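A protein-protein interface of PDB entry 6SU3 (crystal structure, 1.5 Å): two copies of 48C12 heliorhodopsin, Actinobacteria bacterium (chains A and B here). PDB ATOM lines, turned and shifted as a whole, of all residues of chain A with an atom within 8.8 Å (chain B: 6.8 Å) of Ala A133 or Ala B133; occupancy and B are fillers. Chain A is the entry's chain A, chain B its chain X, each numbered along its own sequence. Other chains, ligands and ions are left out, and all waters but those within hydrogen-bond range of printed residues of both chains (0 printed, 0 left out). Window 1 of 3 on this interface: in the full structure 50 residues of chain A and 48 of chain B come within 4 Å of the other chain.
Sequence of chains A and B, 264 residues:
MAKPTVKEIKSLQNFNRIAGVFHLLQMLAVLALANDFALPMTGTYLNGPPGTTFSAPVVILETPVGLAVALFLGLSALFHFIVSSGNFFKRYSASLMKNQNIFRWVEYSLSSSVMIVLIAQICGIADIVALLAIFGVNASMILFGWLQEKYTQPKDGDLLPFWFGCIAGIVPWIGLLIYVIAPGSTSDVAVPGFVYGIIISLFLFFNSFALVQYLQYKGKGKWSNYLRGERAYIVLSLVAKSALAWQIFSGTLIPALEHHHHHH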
ATOM      1  N   SER A 113      20.473 -20.186  13.963  1.00  0.00           N
ATOM      2  CA  SER A 113      20.939 -20.194  12.552  1.00  0.00           C
ATOM      3  C   SER A 113      20.138 -21.225  11.741  1.00  0.00           C
ATOM      4  O   SER A 113      19.728 -20.897  10.636  1.00  0.00           O
ATOM      5  CB  SER A 113      22.428 -20.399  12.473  1.00  0.00           C
ATOM      6  OG  SER A 113      23.113 -19.392  13.225  1.00  0.00           O
ATOM      7  N   ILE A 116      16.657 -19.481  11.249  1.00  0.00           N
ATOM      8  CA  ILE A 116      16.525 -18.387  10.249  1.00  0.00           C
ATOM      9  C   ILE A 116      16.683 -18.980   8.842  1.00  0.00           C
ATOM     10  O   ILE A 116      15.998 -18.514   7.920  1.00  0.00           O
ATOM     11  CB  ILE A 116      17.486 -17.220  10.546  1.00  0.00           C
ATOM     12  CG1 ILE A 116      17.193 -16.022   9.652  1.00  0.00           C
ATOM     13  CG2 ILE A 116      18.940 -17.645  10.448  1.00  0.00           C
ATOM     14  CD1 ILE A 116      15.781 -15.517   9.757  1.00  0.00           C
ATOM     15  N   VAL A 117      17.520 -20.002   8.655  1.00  0.00           N
ATOM     16  CA  VAL A 117      17.602 -20.667   7.325  1.00  0.00           C
ATOM     17  C   VAL A 117      16.228 -21.256   6.974  1.00  0.00           C
ATOM     18  O   VAL A 117      15.790 -21.079   5.824  1.00  0.00           O
ATOM     19  CB  VAL A 117      18.719 -21.720   7.268  1.00  0.00           C
ATOM     20  CG1 VAL A 117      18.604 -22.588   6.013  1.00  0.00           C
ATOM     21  CG2 VAL A 117      20.085 -21.052   7.355  1.00  0.00           C
ATOM     22  N   ILE A 125      13.393 -18.412  -0.376  1.00  0.00           N
ATOM     23  CA  ILE A 125      14.861 -18.285  -0.604  1.00  0.00           C
ATOM     24  C   ILE A 125      15.420 -19.706  -0.717  1.00  0.00           C
ATOM     25  O   ILE A 125      15.145 -20.523   0.177  1.00  0.00           O
ATOM     26  CB  ILE A 125      15.543 -17.433   0.484  1.00  0.00           C
ATOM     27  CG1 ILE A 125      14.927 -16.029   0.529  1.00  0.00           C
ATOM     28  CG2 ILE A 125      17.045 -17.383   0.244  1.00  0.00           C
ATOM     29  CD1 ILE A 125      15.300 -15.205   1.740  1.00  0.00           C
ATOM     30  N   ASP A 127      18.568 -20.341  -3.038  1.00  0.00           N
ATOM     31  CA  ASP A 127      19.977 -20.341  -3.491  1.00  0.00           C
ATOM     32  C   ASP A 127      20.864 -20.828  -2.339  1.00  0.00           C
ATOM     33  O   ASP A 127      20.770 -20.277  -1.218  1.00  0.00           O
ATOM     34  CB  ASP A 127      20.432 -18.963  -3.965  1.00  0.00           C
ATOM     35  CG  ASP A 127      21.834 -19.034  -4.535  1.00  0.00           C
ATOM     36  OD1 ASP A 127      22.774 -18.848  -3.746  1.00  0.00           O
ATOM     37  OD2 ASP A 127      21.966 -19.341  -5.759  1.00  0.00           O
ATOM     38  N   ILE A 128      21.714 -21.815  -2.593  1.00  0.00           N
ATOM     39  CA  ILE A 128      22.468 -22.502  -1.510  1.00  0.00           C
ATOM     40  C   ILE A 128      23.433 -21.497  -0.865  1.00  0.00           C
ATOM     41  O   ILE A 128      23.689 -21.616   0.330  1.00  0.00           O
ATOM     42  CB  ILE A 128      23.170 -23.764  -2.053  1.00  0.00           C
ATOM     43  CG1 ILE A 128      23.750 -24.604  -0.915  1.00  0.00           C
ATOM     44  CG2 ILE A 128      24.217 -23.404  -3.095  1.00  0.00           C
ATOM     45  CD1 ILE A 128      24.195 -25.994  -1.325  1.00  0.00           C
ATOM     46  N   VAL A 129      23.936 -20.517  -1.618  1.00  0.00           N
ATOM     47  CA  VAL A 129      24.879 -19.504  -1.069  1.00  0.00           C
ATOM     48  C   VAL A 129      24.091 -18.494  -0.226  1.00  0.00           C
ATOM     49  O   VAL A 129      24.605 -18.068   0.835  1.00  0.00           O
ATOM     50  CB  VAL A 129      25.701 -18.828  -2.182  1.00  0.00           C
ATOM     51  CG1 VAL A 129      26.630 -17.758  -1.619  1.00  0.00           C
ATOM     52  CG2 VAL A 129      26.490 -19.867  -2.963  1.00  0.00           C
ATOM     53  N   ALA A 130      22.892 -18.108  -0.658  1.00  0.00           N
ATOM     54  CA  ALA A 130      21.991 -17.284   0.179  1.00  0.00           C
ATOM     55  C   ALA A 130      21.824 -17.987   1.530  1.00  0.00           C
ATOM     56  O   ALA A 130      21.975 -17.333   2.555  1.00  0.00           O
ATOM     57  CB  ALA A 130      20.670 -17.041  -0.515  1.00  0.00           C
ATOM     58  N   LEU A 131      21.514 -19.286   1.542  1.00  0.00           N
ATOM     59  CA  LEU A 131      21.205 -19.988   2.809  1.00  0.00           C
ATOM     60  C   LEU A 131      22.482 -20.148   3.642  1.00  0.00           C
ATOM     61  O   LEU A 131      22.420 -19.942   4.868  1.00  0.00           O
ATOM     62  CB  LEU A 131      20.528 -21.318   2.491  1.00  0.00           C
ATOM     63  CG  LEU A 131      19.213 -21.181   1.722  1.00  0.00           C
ATOM     64  CD1 LEU A 131      18.627 -22.542   1.406  1.00  0.00           C
ATOM     65  CD2 LEU A 131      18.206 -20.337   2.484  1.00  0.00           C
ATOM     66  N   LEU A 132      23.602 -20.488   3.011  1.00  0.00           N
ATOM     67  CA  LEU A 132      24.911 -20.595   3.700  1.00  0.00           C
ATOM     68  C   LEU A 132      25.274 -19.244   4.334  1.00  0.00           C
ATOM     69  O   LEU A 132      25.670 -19.218   5.513  1.00  0.00           O
ATOM     70  CB  LEU A 132      25.966 -21.032   2.684  1.00  0.00           C
ATOM     71  CG  LEU A 132      27.412 -20.987   3.171  1.00  0.00           C
ATOM     72  CD1 LEU A 132      27.641 -21.984   4.291  1.00  0.00           C
ATOM     73  CD2 LEU A 132      28.367 -21.240   2.021  1.00  0.00           C
ATOM     74  N   ALA A 133      25.143 -18.149   3.588  1.00  0.00           N
ATOM     75  CA  ALA A 133      25.582 -16.816   4.055  1.00  0.00           C
ATOM     76  C   ALA A 133      24.603 -16.315   5.130  1.00  0.00           C
ATOM     77  O   ALA A 133      25.041 -15.686   6.096  1.00  0.00           O
ATOM     78  CB  ALA A 133      25.710 -15.852   2.906  1.00  0.00           C
ATOM     79  N   ILE A 134      23.318 -16.635   5.009  1.00  0.00           N
ATOM     80  CA  ILE A 134      22.338 -16.349   6.097  1.00  0.00           C
ATOM     81  C   ILE A 134      22.783 -17.073   7.372  1.00  0.00           C
ATOM     82  O   ILE A 134      22.819 -16.433   8.447  1.00  0.00           O
ATOM     83  CB  ILE A 134      20.909 -16.726   5.670  1.00  0.00           C
ATOM     84  CG1 ILE A 134      20.332 -15.653   4.742  1.00  0.00           C
ATOM     85  CG2 ILE A 134      20.050 -16.962   6.904  1.00  0.00           C
ATOM     86  CD1 ILE A 134      19.039 -16.052   4.072  1.00  0.00           C
ATOM     87  N   PHE A 135      23.146 -18.348   7.272  1.00  0.00           N
ATOM     88  CA  PHE A 135      23.613 -19.133   8.439  1.00  0.00           C
ATOM     89  C   PHE A 135      24.830 -18.421   9.046  1.00  0.00           C
ATOM     90  O   PHE A 135      24.870 -18.202  10.281  1.00  0.00           O
ATOM     91  CB  PHE A 135      23.912 -20.578   8.040  1.00  0.00           C
ATOM     92  CG  PHE A 135      24.042 -21.516   9.217  1.00  0.00           C
ATOM     93  CD1 PHE A 135      25.164 -21.491  10.029  1.00  0.00           C
ATOM     94  CD2 PHE A 135      23.031 -22.412   9.527  1.00  0.00           C
ATOM     95  CE1 PHE A 135      25.276 -22.352  11.110  1.00  0.00           C
ATOM     96  CE2 PHE A 135      23.141 -23.265  10.613  1.00  0.00           C
ATOM     97  CZ  PHE A 135      24.266 -23.237  11.399  1.00  0.00           C
ATOM     98  N   GLY A 136      25.789 -18.031   8.205  1.00  0.00           N
ATOM     99  CA  GLY A 136      27.049 -17.409   8.654  1.00  0.00           C
ATOM    100  C   GLY A 136      26.809 -16.064   9.317  1.00  0.00           C
ATOM    101  O   GLY A 136      27.426 -15.785  10.356  1.00  0.00           O
ATOM    102  N   VAL A 137      25.986 -15.209   8.717  1.00  0.00           N
ATOM    103  CA  VAL A 137      25.784 -13.833   9.263  1.00  0.00           C
ATOM    104  C   VAL A 137      24.937 -13.903  10.545  1.00  0.00           C
ATOM    105  O   VAL A 137      25.176 -13.123  11.487  1.00  0.00           O
ATOM    106  CB  VAL A 137      25.197 -12.881   8.212  1.00  0.00           C
ATOM    107  CG1 VAL A 137      23.698 -13.069   8.025  1.00  0.00           C
ATOM    108  CG2 VAL A 137      25.546 -11.443   8.553  1.00  0.00           C
ATOM    109  N   ASN A 138      24.016 -14.857  10.630  1.00  0.00           N
ATOM    110  CA  ASN A 138      23.228 -15.081  11.867  1.00  0.00           C
ATOM    111  C   ASN A 138      24.155 -15.619  12.978  1.00  0.00           C
ATOM    112  O   ASN A 138      24.082 -15.126  14.132  1.00  0.00           O
ATOM    113  CB  ASN A 138      22.047 -16.016  11.615  1.00  0.00           C
ATOM    114  CG  ASN A 138      21.149 -16.066  12.827  1.00  0.00           C
ATOM    115  OD1 ASN A 138      20.283 -15.209  12.975  1.00  0.00           O
ATOM    116  ND2 ASN A 138      21.391 -17.024  13.714  1.00  0.00           N
ATOM    117  N   ALA A 139      25.016 -16.592  12.666  1.00  0.00           N
ATOM    118  CA  ALA A 139      26.031 -17.091  13.623  1.00  0.00           C
ATOM    119  C   ALA A 139      26.884 -15.920  14.117  1.00  0.00           C
ATOM    120  O   ALA A 139      27.165 -15.840  15.339  1.00  0.00           O
ATOM    121  CB  ALA A 139      26.876 -18.169  13.000  1.00  0.00           C
ATOM    122  N   SER A 140      27.272 -15.031  13.202  1.00  0.00           N
ATOM    123  CA  SER A 140      28.096 -13.840  13.510  1.00  0.00           C
ATOM    124  C   SER A 140      27.369 -12.973  14.543  1.00  0.00           C
ATOM    125  O   SER A 140      27.997 -12.545  15.516  1.00  0.00           O
ATOM    126  CB  SER A 140      28.409 -13.070  12.243  1.00  0.00           C
ATOM    127  OG  SER A 140      29.295 -13.809  11.407  1.00  0.00           O
ATOM    128  N   ALA A 168      24.881  -7.349  11.872  1.00  0.00           N
ATOM    129  CA  ALA A 168      24.909  -8.711  11.312  1.00  0.00           C
ATOM    130  C   ALA A 168      23.482  -9.277  11.376  1.00  0.00           C
ATOM    131  O   ALA A 168      23.015  -9.883  10.375  1.00  0.00           O
ATOM    132  CB  ALA A 168      25.892  -9.552  12.078  1.00  0.00           C
ATOM    133  N   ILE A 170      20.426  -8.128  11.463  1.00  0.00           N
ATOM    134  CA  ILE A 170      19.271  -7.595  10.687  1.00  0.00           C
ATOM    135  C   ILE A 170      19.360  -8.087   9.235  1.00  0.00           C
ATOM    136  O   ILE A 170      18.330  -8.077   8.540  1.00  0.00           O
ATOM    137  CB  ILE A 170      19.188  -6.066  10.795  1.00  0.00           C
ATOM    138  CG1 ILE A 170      17.790  -5.562  10.425  1.00  0.00           C
ATOM    139  CG2 ILE A 170      20.278  -5.392   9.978  1.00  0.00           C
ATOM    140  CD1 ILE A 170      16.686  -6.083  11.310  1.00  0.00           C
ATOM    141  N   VAL A 171      20.529  -8.550   8.792  1.00  0.00           N
ATOM    142  CA  VAL A 171      20.773  -8.842   7.350  1.00  0.00           C
ATOM    143  C   VAL A 171      19.790  -9.898   6.847  1.00  0.00           C
ATOM    144  O   VAL A 171      19.177  -9.699   5.801  1.00  0.00           O
ATOM    145  CB  VAL A 171      22.244  -9.206   7.080  1.00  0.00           C
ATOM    146  CG1 VAL A 171      22.439  -9.836   5.712  1.00  0.00           C
ATOM    147  CG2 VAL A 171      23.124  -7.971   7.210  1.00  0.00           C
ATOM    148  N   PRO A 172      19.604 -11.061   7.519  1.00  0.00           N
ATOM    149  CA  PRO A 172      18.678 -12.069   7.004  1.00  0.00           C
ATOM    150  C   PRO A 172      17.251 -11.528   6.865  1.00  0.00           C
ATOM    151  O   PRO A 172      16.552 -11.920   5.955  1.00  0.00           O
ATOM    152  CB  PRO A 172      18.726 -13.199   8.039  1.00  0.00           C
ATOM    153  CG  PRO A 172      20.078 -13.016   8.711  1.00  0.00           C
ATOM    154  CD  PRO A 172      20.306 -11.515   8.732  1.00  0.00           C
ATOM    155  N   TRP A 173      16.855 -10.661   7.797  1.00  0.00           N
ATOM    156  CA  TRP A 173      15.478 -10.113   7.883  1.00  0.00           C
ATOM    157  C   TRP A 173      15.256  -9.128   6.726  1.00  0.00           C
ATOM    158  O   TRP A 173      14.152  -9.115   6.152  1.00  0.00           O
ATOM    159  CB  TRP A 173      15.254  -9.514   9.279  1.00  0.00           C
ATOM    160  CG  TRP A 173      15.337 -10.593  10.316  1.00  0.00           C
ATOM    161  CD1 TRP A 173      16.456 -10.988  10.990  1.00  0.00           C
ATOM    162  CD2 TRP A 173      14.305 -11.527  10.682  1.00  0.00           C
ATOM    163  NE1 TRP A 173      16.181 -12.070  11.778  1.00  0.00           N
ATOM    164  CE2 TRP A 173      14.865 -12.412  11.628  1.00  0.00           C
ATOM    165  CE3 TRP A 173      12.949 -11.653  10.366  1.00  0.00           C
ATOM    166  CZ2 TRP A 173      14.129 -13.434  12.224  1.00  0.00           C
ATOM    167  CZ3 TRP A 173      12.227 -12.676  10.943  1.00  0.00           C
ATOM    168  CH2 TRP A 173      12.807 -13.549  11.856  1.00  0.00           C
ATOM    169  N   ILE A 174      16.278  -8.358   6.352  1.00  0.00           N
ATOM    170  CA  ILE A 174      16.211  -7.533   5.116  1.00  0.00           C
ATOM    171  C   ILE A 174      16.003  -8.485   3.931  1.00  0.00           C
ATOM    172  O   ILE A 174      15.174  -8.193   3.063  1.00  0.00           O
ATOM    173  CB  ILE A 174      17.463  -6.645   4.969  1.00  0.00           C
ATOM    174  CG1 ILE A 174      17.568  -5.656   6.131  1.00  0.00           C
ATOM    175  CG2 ILE A 174      17.468  -5.956   3.606  1.00  0.00           C
ATOM    176  CD1 ILE A 174      18.865  -4.875   6.182  1.00  0.00           C
ATOM    177  N   GLY A 175      16.708  -9.616   3.919  1.00  0.00           N
ATOM    178  CA  GLY A 175      16.544 -10.637   2.864  1.00  0.00           C
ATOM    179  C   GLY A 175      15.106 -11.134   2.795  1.00  0.00           C
ATOM    180  O   GLY A 175      14.561 -11.206   1.672  1.00  0.00           O
ATOM    181  N   ILE A 178      12.794  -8.443   1.347  1.00  0.00           N
ATOM    182  CA  ILE A 178      12.968  -8.370  -0.132  1.00  0.00           C
ATOM    183  C   ILE A 178      12.126  -9.479  -0.775  1.00  0.00           C
ATOM    184  O   ILE A 178      11.443  -9.196  -1.768  1.00  0.00           O
ATOM    185  CB  ILE A 178      14.446  -8.445  -0.543  1.00  0.00           C
ATOM    186  CG1 ILE A 178      15.233  -7.220  -0.066  1.00  0.00           C
ATOM    187  CG2 ILE A 178      14.566  -8.646  -2.042  1.00  0.00           C
ATOM    188  CD1 ILE A 178      16.747  -7.386  -0.132  1.00  0.00           C
ATOM    189  N   ILE B 128      19.852 -11.931  -4.832  1.00  0.00           N
ATOM    190  CA  ILE B 128      20.094 -10.640  -4.130  1.00  0.00           C
ATOM    191  C   ILE B 128      20.340 -10.935  -2.648  1.00  0.00           C
ATOM    192  O   ILE B 128      21.118 -10.215  -2.018  1.00  0.00           O
ATOM    193  CB  ILE B 128      18.929  -9.658  -4.357  1.00  0.00           C
ATOM    194  CG1 ILE B 128      19.265  -8.263  -3.828  1.00  0.00           C
ATOM    195  CG2 ILE B 128      17.630 -10.191  -3.769  1.00  0.00           C
ATOM    196  CD1 ILE B 128      18.360  -7.178  -4.351  1.00  0.00           C
ATOM    197  N   VAL B 129      19.702 -11.969  -2.097  1.00  0.00           N
ATOM    198  CA  VAL B 129      19.898 -12.310  -0.666  1.00  0.00           C
ATOM    199  C   VAL B 129      21.280 -12.950  -0.502  1.00  0.00           C
ATOM    200  O   VAL B 129      21.942 -12.660   0.520  1.00  0.00           O
ATOM    201  CB  VAL B 129      18.763 -13.190  -0.118  1.00  0.00           C
ATOM    202  CG1 VAL B 129      19.027 -13.559   1.336  1.00  0.00           C
ATOM    203  CG2 VAL B 129      17.429 -12.470  -0.263  1.00  0.00           C
ATOM    204  N   ALA B 130      21.726 -13.771  -1.459  1.00  0.00           N
ATOM    205  CA  ALA B 130      23.095 -14.335  -1.438  1.00  0.00           C
ATOM    206  C   ALA B 130      24.090 -13.174  -1.396  1.00  0.00           C
ATOM    207  O   ALA B 130      25.034 -13.225  -0.589  1.00  0.00           O
ATOM    208  CB  ALA B 130      23.339 -15.239  -2.626  1.00  0.00           C
ATOM    209  N   LEU B 131      23.900 -12.151  -2.231  1.00  0.00           N
ATOM    210  CA  LEU B 131      24.879 -11.030  -2.324  1.00  0.00           C
ATOM    211  C   LEU B 131      24.805 -10.161  -1.060  1.00  0.00           C
ATOM    212  O   LEU B 131      25.863  -9.790  -0.544  1.00  0.00           O
ATOM    213  CB  LEU B 131      24.614 -10.235  -3.600  1.00  0.00           C
ATOM    214  CG  LEU B 131      24.777 -11.057  -4.881  1.00  0.00           C
ATOM    215  CD1 LEU B 131      24.461 -10.225  -6.106  1.00  0.00           C
ATOM    216  CD2 LEU B 131      26.176 -11.649  -4.982  1.00  0.00           C
ATOM    217  N   LEU B 132      23.599  -9.860  -0.574  1.00  0.00           N
ATOM    218  CA  LEU B 132      23.375  -9.110   0.683  1.00  0.00           C
ATOM    219  C   LEU B 132      24.036  -9.849   1.854  1.00  0.00           C
ATOM    220  O   LEU B 132      24.775  -9.210   2.632  1.00  0.00           O
ATOM    221  CB  LEU B 132      21.868  -8.969   0.906  1.00  0.00           C
ATOM    222  CG  LEU B 132      21.472  -8.345   2.240  1.00  0.00           C
ATOM    223  CD1 LEU B 132      22.017  -6.930   2.344  1.00  0.00           C
ATOM    224  CD2 LEU B 132      19.962  -8.363   2.422  1.00  0.00           C
ATOM    225  N   ALA B 133      23.784 -11.148   1.997  1.00  0.00           N
ATOM    226  CA  ALA B 133      24.287 -11.936   3.139  1.00  0.00           C
ATOM    227  C   ALA B 133      25.814 -12.114   3.022  1.00  0.00           C
ATOM    228  O   ALA B 133      26.513 -12.111   4.067  1.00  0.00           O
ATOM    229  CB  ALA B 133      23.559 -13.252   3.232  1.00  0.00           C
ATOM    230  N   ILE B 134      26.345 -12.212   1.805  1.00  0.00           N
ATOM    231  CA  ILE B 134      27.824 -12.246   1.591  1.00  0.00           C
ATOM    232  C   ILE B 134      28.406 -10.911   2.070  1.00  0.00           C
ATOM    233  O   ILE B 134      29.411 -10.905   2.804  1.00  0.00           O
ATOM    234  CB  ILE B 134      28.182 -12.558   0.121  1.00  0.00           C
ATOM    235  CG1 ILE B 134      28.024 -14.054  -0.177  1.00  0.00           C
ATOM    236  CG2 ILE B 134      29.583 -12.058  -0.199  1.00  0.00           C
ATOM    237  CD1 ILE B 134      28.062 -14.398  -1.656  1.00  0.00           C
ATOM    238  N   PHE B 135      27.796  -9.797   1.676  1.00  0.00           N
ATOM    239  CA  PHE B 135      28.250  -8.459   2.121  1.00  0.00           C
ATOM    240  C   PHE B 135      28.243  -8.426   3.658  1.00  0.00           C
ATOM    241  O   PHE B 135      29.250  -7.999   4.263  1.00  0.00           O
ATOM    242  CB  PHE B 135      27.379  -7.356   1.527  1.00  0.00           C
ATOM    243  CG  PHE B 135      27.963  -5.971   1.663  1.00  0.00           C
ATOM    244  CD1 PHE B 135      28.542  -5.346   0.574  1.00  0.00           C
ATOM    245  CD2 PHE B 135      27.981  -5.313   2.886  1.00  0.00           C
ATOM    246  CE1 PHE B 135      29.091  -4.081   0.690  1.00  0.00           C
ATOM    247  CE2 PHE B 135      28.533  -4.046   2.998  1.00  0.00           C
ATOM    248  CZ  PHE B 135      29.090  -3.437   1.905  1.00  0.00           C
ATOM    249  N   GLY B 136      27.146  -8.865   4.283  1.00  0.00           N
ATOM    250  CA  GLY B 136      27.005  -8.834   5.758  1.00  0.00           C
ATOM    251  C   GLY B 136      28.032  -9.712   6.461  1.00  0.00           C
ATOM    252  O   GLY B 136      28.581  -9.291   7.501  1.00  0.00           O
ATOM    253  N   VAL B 137      28.231 -10.942   5.990  1.00  0.00           N
ATOM    254  CA  VAL B 137      29.127 -11.895   6.707  1.00  0.00           C
ATOM    255  C   VAL B 137      30.582 -11.457   6.495  1.00  0.00           C
ATOM    256  O   VAL B 137      31.403 -11.613   7.422  1.00  0.00           O
ATOM    257  CB  VAL B 137      28.864 -13.363   6.326  1.00  0.00           C
ATOM    258  CG1 VAL B 137      29.454 -13.747   4.976  1.00  0.00           C
ATOM    259  CG2 VAL B 137      29.360 -14.296   7.422  1.00  0.00           C
ATOM    260  N   ASN B 138      30.896 -10.884   5.336  1.00  0.00           N
ATOM    261  CA  ASN B 138      32.234 -10.300   5.069  1.00  0.00           C
ATOM    262  C   ASN B 138      32.452  -9.078   5.973  1.00  0.00           C
ATOM    263  O   ASN B 138      33.535  -8.968   6.594  1.00  0.00           O
ATOM    264  CB  ASN B 138      32.429  -9.948   3.596  1.00  0.00           C
ATOM    265  CG  ASN B 138      33.869  -9.571   3.326  1.00  0.00           C
ATOM    266  OD1 ASN B 138      34.695 -10.449   3.097  1.00  0.00           O
ATOM    267  ND2 ASN B 138      34.179  -8.282   3.392  1.00  0.00           N
ATOM    268  N   ALA B 139      31.471  -8.180   6.071  1.00  0.00           N
ATOM    269  CA  ALA B 139      31.557  -7.031   6.997  1.00  0.00           C
ATOM    270  C   ALA B 139      31.791  -7.562   8.415  1.00  0.00           C
ATOM    271  O   ALA B 139      32.612  -6.978   9.135  1.00  0.00           O
ATOM    272  CB  ALA B 139      30.322  -6.162   6.905  1.00  0.00           C
ATOM    273  N   VAL B 171      33.061 -17.977   4.891  1.00  0.00           N
ATOM    274  CA  VAL B 171      31.708 -18.366   4.394  1.00  0.00           C
ATOM    275  C   VAL B 171      31.567 -17.975   2.924  1.00  0.00           C
ATOM    276  O   VAL B 171      31.146 -18.795   2.116  1.00  0.00           O
ATOM    277  CB  VAL B 171      30.608 -17.782   5.291  1.00  0.00           C
ATOM    278  CG1 VAL B 171      29.238 -17.860   4.629  1.00  0.00           C
ATOM    279  CG2 VAL B 171      30.601 -18.499   6.634  1.00  0.00           C
ATOM    280  N   PRO B 172      31.880 -16.727   2.494  1.00  0.00           N
ATOM    281  CA  PRO B 172      31.716 -16.373   1.085  1.00  0.00           C
ATOM    282  C   PRO B 172      32.530 -17.293   0.159  1.00  0.00           C
ATOM    283  O   PRO B 172      32.072 -17.605  -0.930  1.00  0.00           O
ATOM    284  CB  PRO B 172      32.186 -14.916   0.999  1.00  0.00           C
ATOM    285  CG  PRO B 172      32.033 -14.390   2.426  1.00  0.00           C
ATOM    286  CD  PRO B 172      32.325 -15.586   3.313  1.00  0.00           C
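The backbone NH of Ala A130 lies within hydrogen-bond range of the side-chain carboxylate of Asp A127.
The backbone carbonyl oxygen (O) of Gly A136 lies within hydrogen-bond range of the side-chain hydroxyl (OG) of Ser A140 (2.9 Å).
The side-chain carboxylate of Asp A127 is in hydrogen-bond range of the backbone NH of Val A129.
Among the printed residues, pairs that only touch across the chains: Asp A127 with Ala B130 (3.8 Å), Val A129 with Ile B134 (3.7 Å), Ala A130 with Ala B130 (3.5 Å), Leu A132 with Val B171 (3.7 Å), Ala A133 with Ala B133 (3.4 Å), Ala A133 with Ile B134 (3.9 Å), Ala A133 with Val B171 (3.8 Å), Ile A134 with Val B129 (3.7 Å), Ile A134 with Ala B133 (3.8 Å), Gly A136 with Val B137 (3.6 Å), Val A137 with Gly B136 (3.7 Å), Val A137 with Val B137 (3.7 Å), Val A171 with Leu B132 (3.7 Å), Val A171 with Ala B133 (3.8 Å), Ile A174 with Leu B132 (3.7 Å), Gly A175 with Val B129 (3.7 Å), Gly A175 with Leu B132 (3.8 Å) and Ile A178 with Ile B128 (3.8 Å).
Ala A133 touches just these residues of chain B: Ala B133 (3.4 Å), Ile B134 (3.9 Å) and Val B171 (3.8 Å).
Of the printed residues of chain B, Ile A134 touches Val B129 (3.7 Å) and Ala B133 (3.8 Å).
Printed residues of chain B within 4 Å of Val A171: Leu B132 and Ala B133.
Of the printed residues of chain B, Gly A175 touches Val B129 (3.7 Å) and Leu B132 (3.8 Å).
Of chain A, only Val A171, Ile A174 and Gly A175 come within 4 Å of Leu B132.
Of chain A, only Ala A133, Ile A134 and Val A171 come within 4 Å of Ala B133.
Ala B139 touches none of the printed residues of chain A.
The nearest residue of chain B that does not touch Ala A133 is Ala B130 (4.4 Å).
Hydrophobic or aromatic side chains of chain A within 4 Å of the printed part of chain B: Val A129, Ala A130, Leu A132, Ala A133, Ile A134, Val A137, Val A171, Ile A174 and Ile A178.
Hydrophobic or aromatic side chains of chain B that line the printed part of chain A: Ile B128, Val B129, Ala B130, Leu B132, Ala B133, Ile B134, Val B137 and Val B171.
Among the printed residues, no Asp or Glu carboxylate lies within 4 Å of a Lys or Arg side-chain nitrogen of the other chain.
Val A129 touches Ile B134, and with the chains exchanged Ile A134 touches Val B129.
Leu A132 touches Val B171, and with the chains exchanged Val A171 touches Leu B132.
Ala A133 touches Ile B134, and with the chains exchanged Ile A134 touches Ala B133.
Val B137 touches its own counterpart, Val A137.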
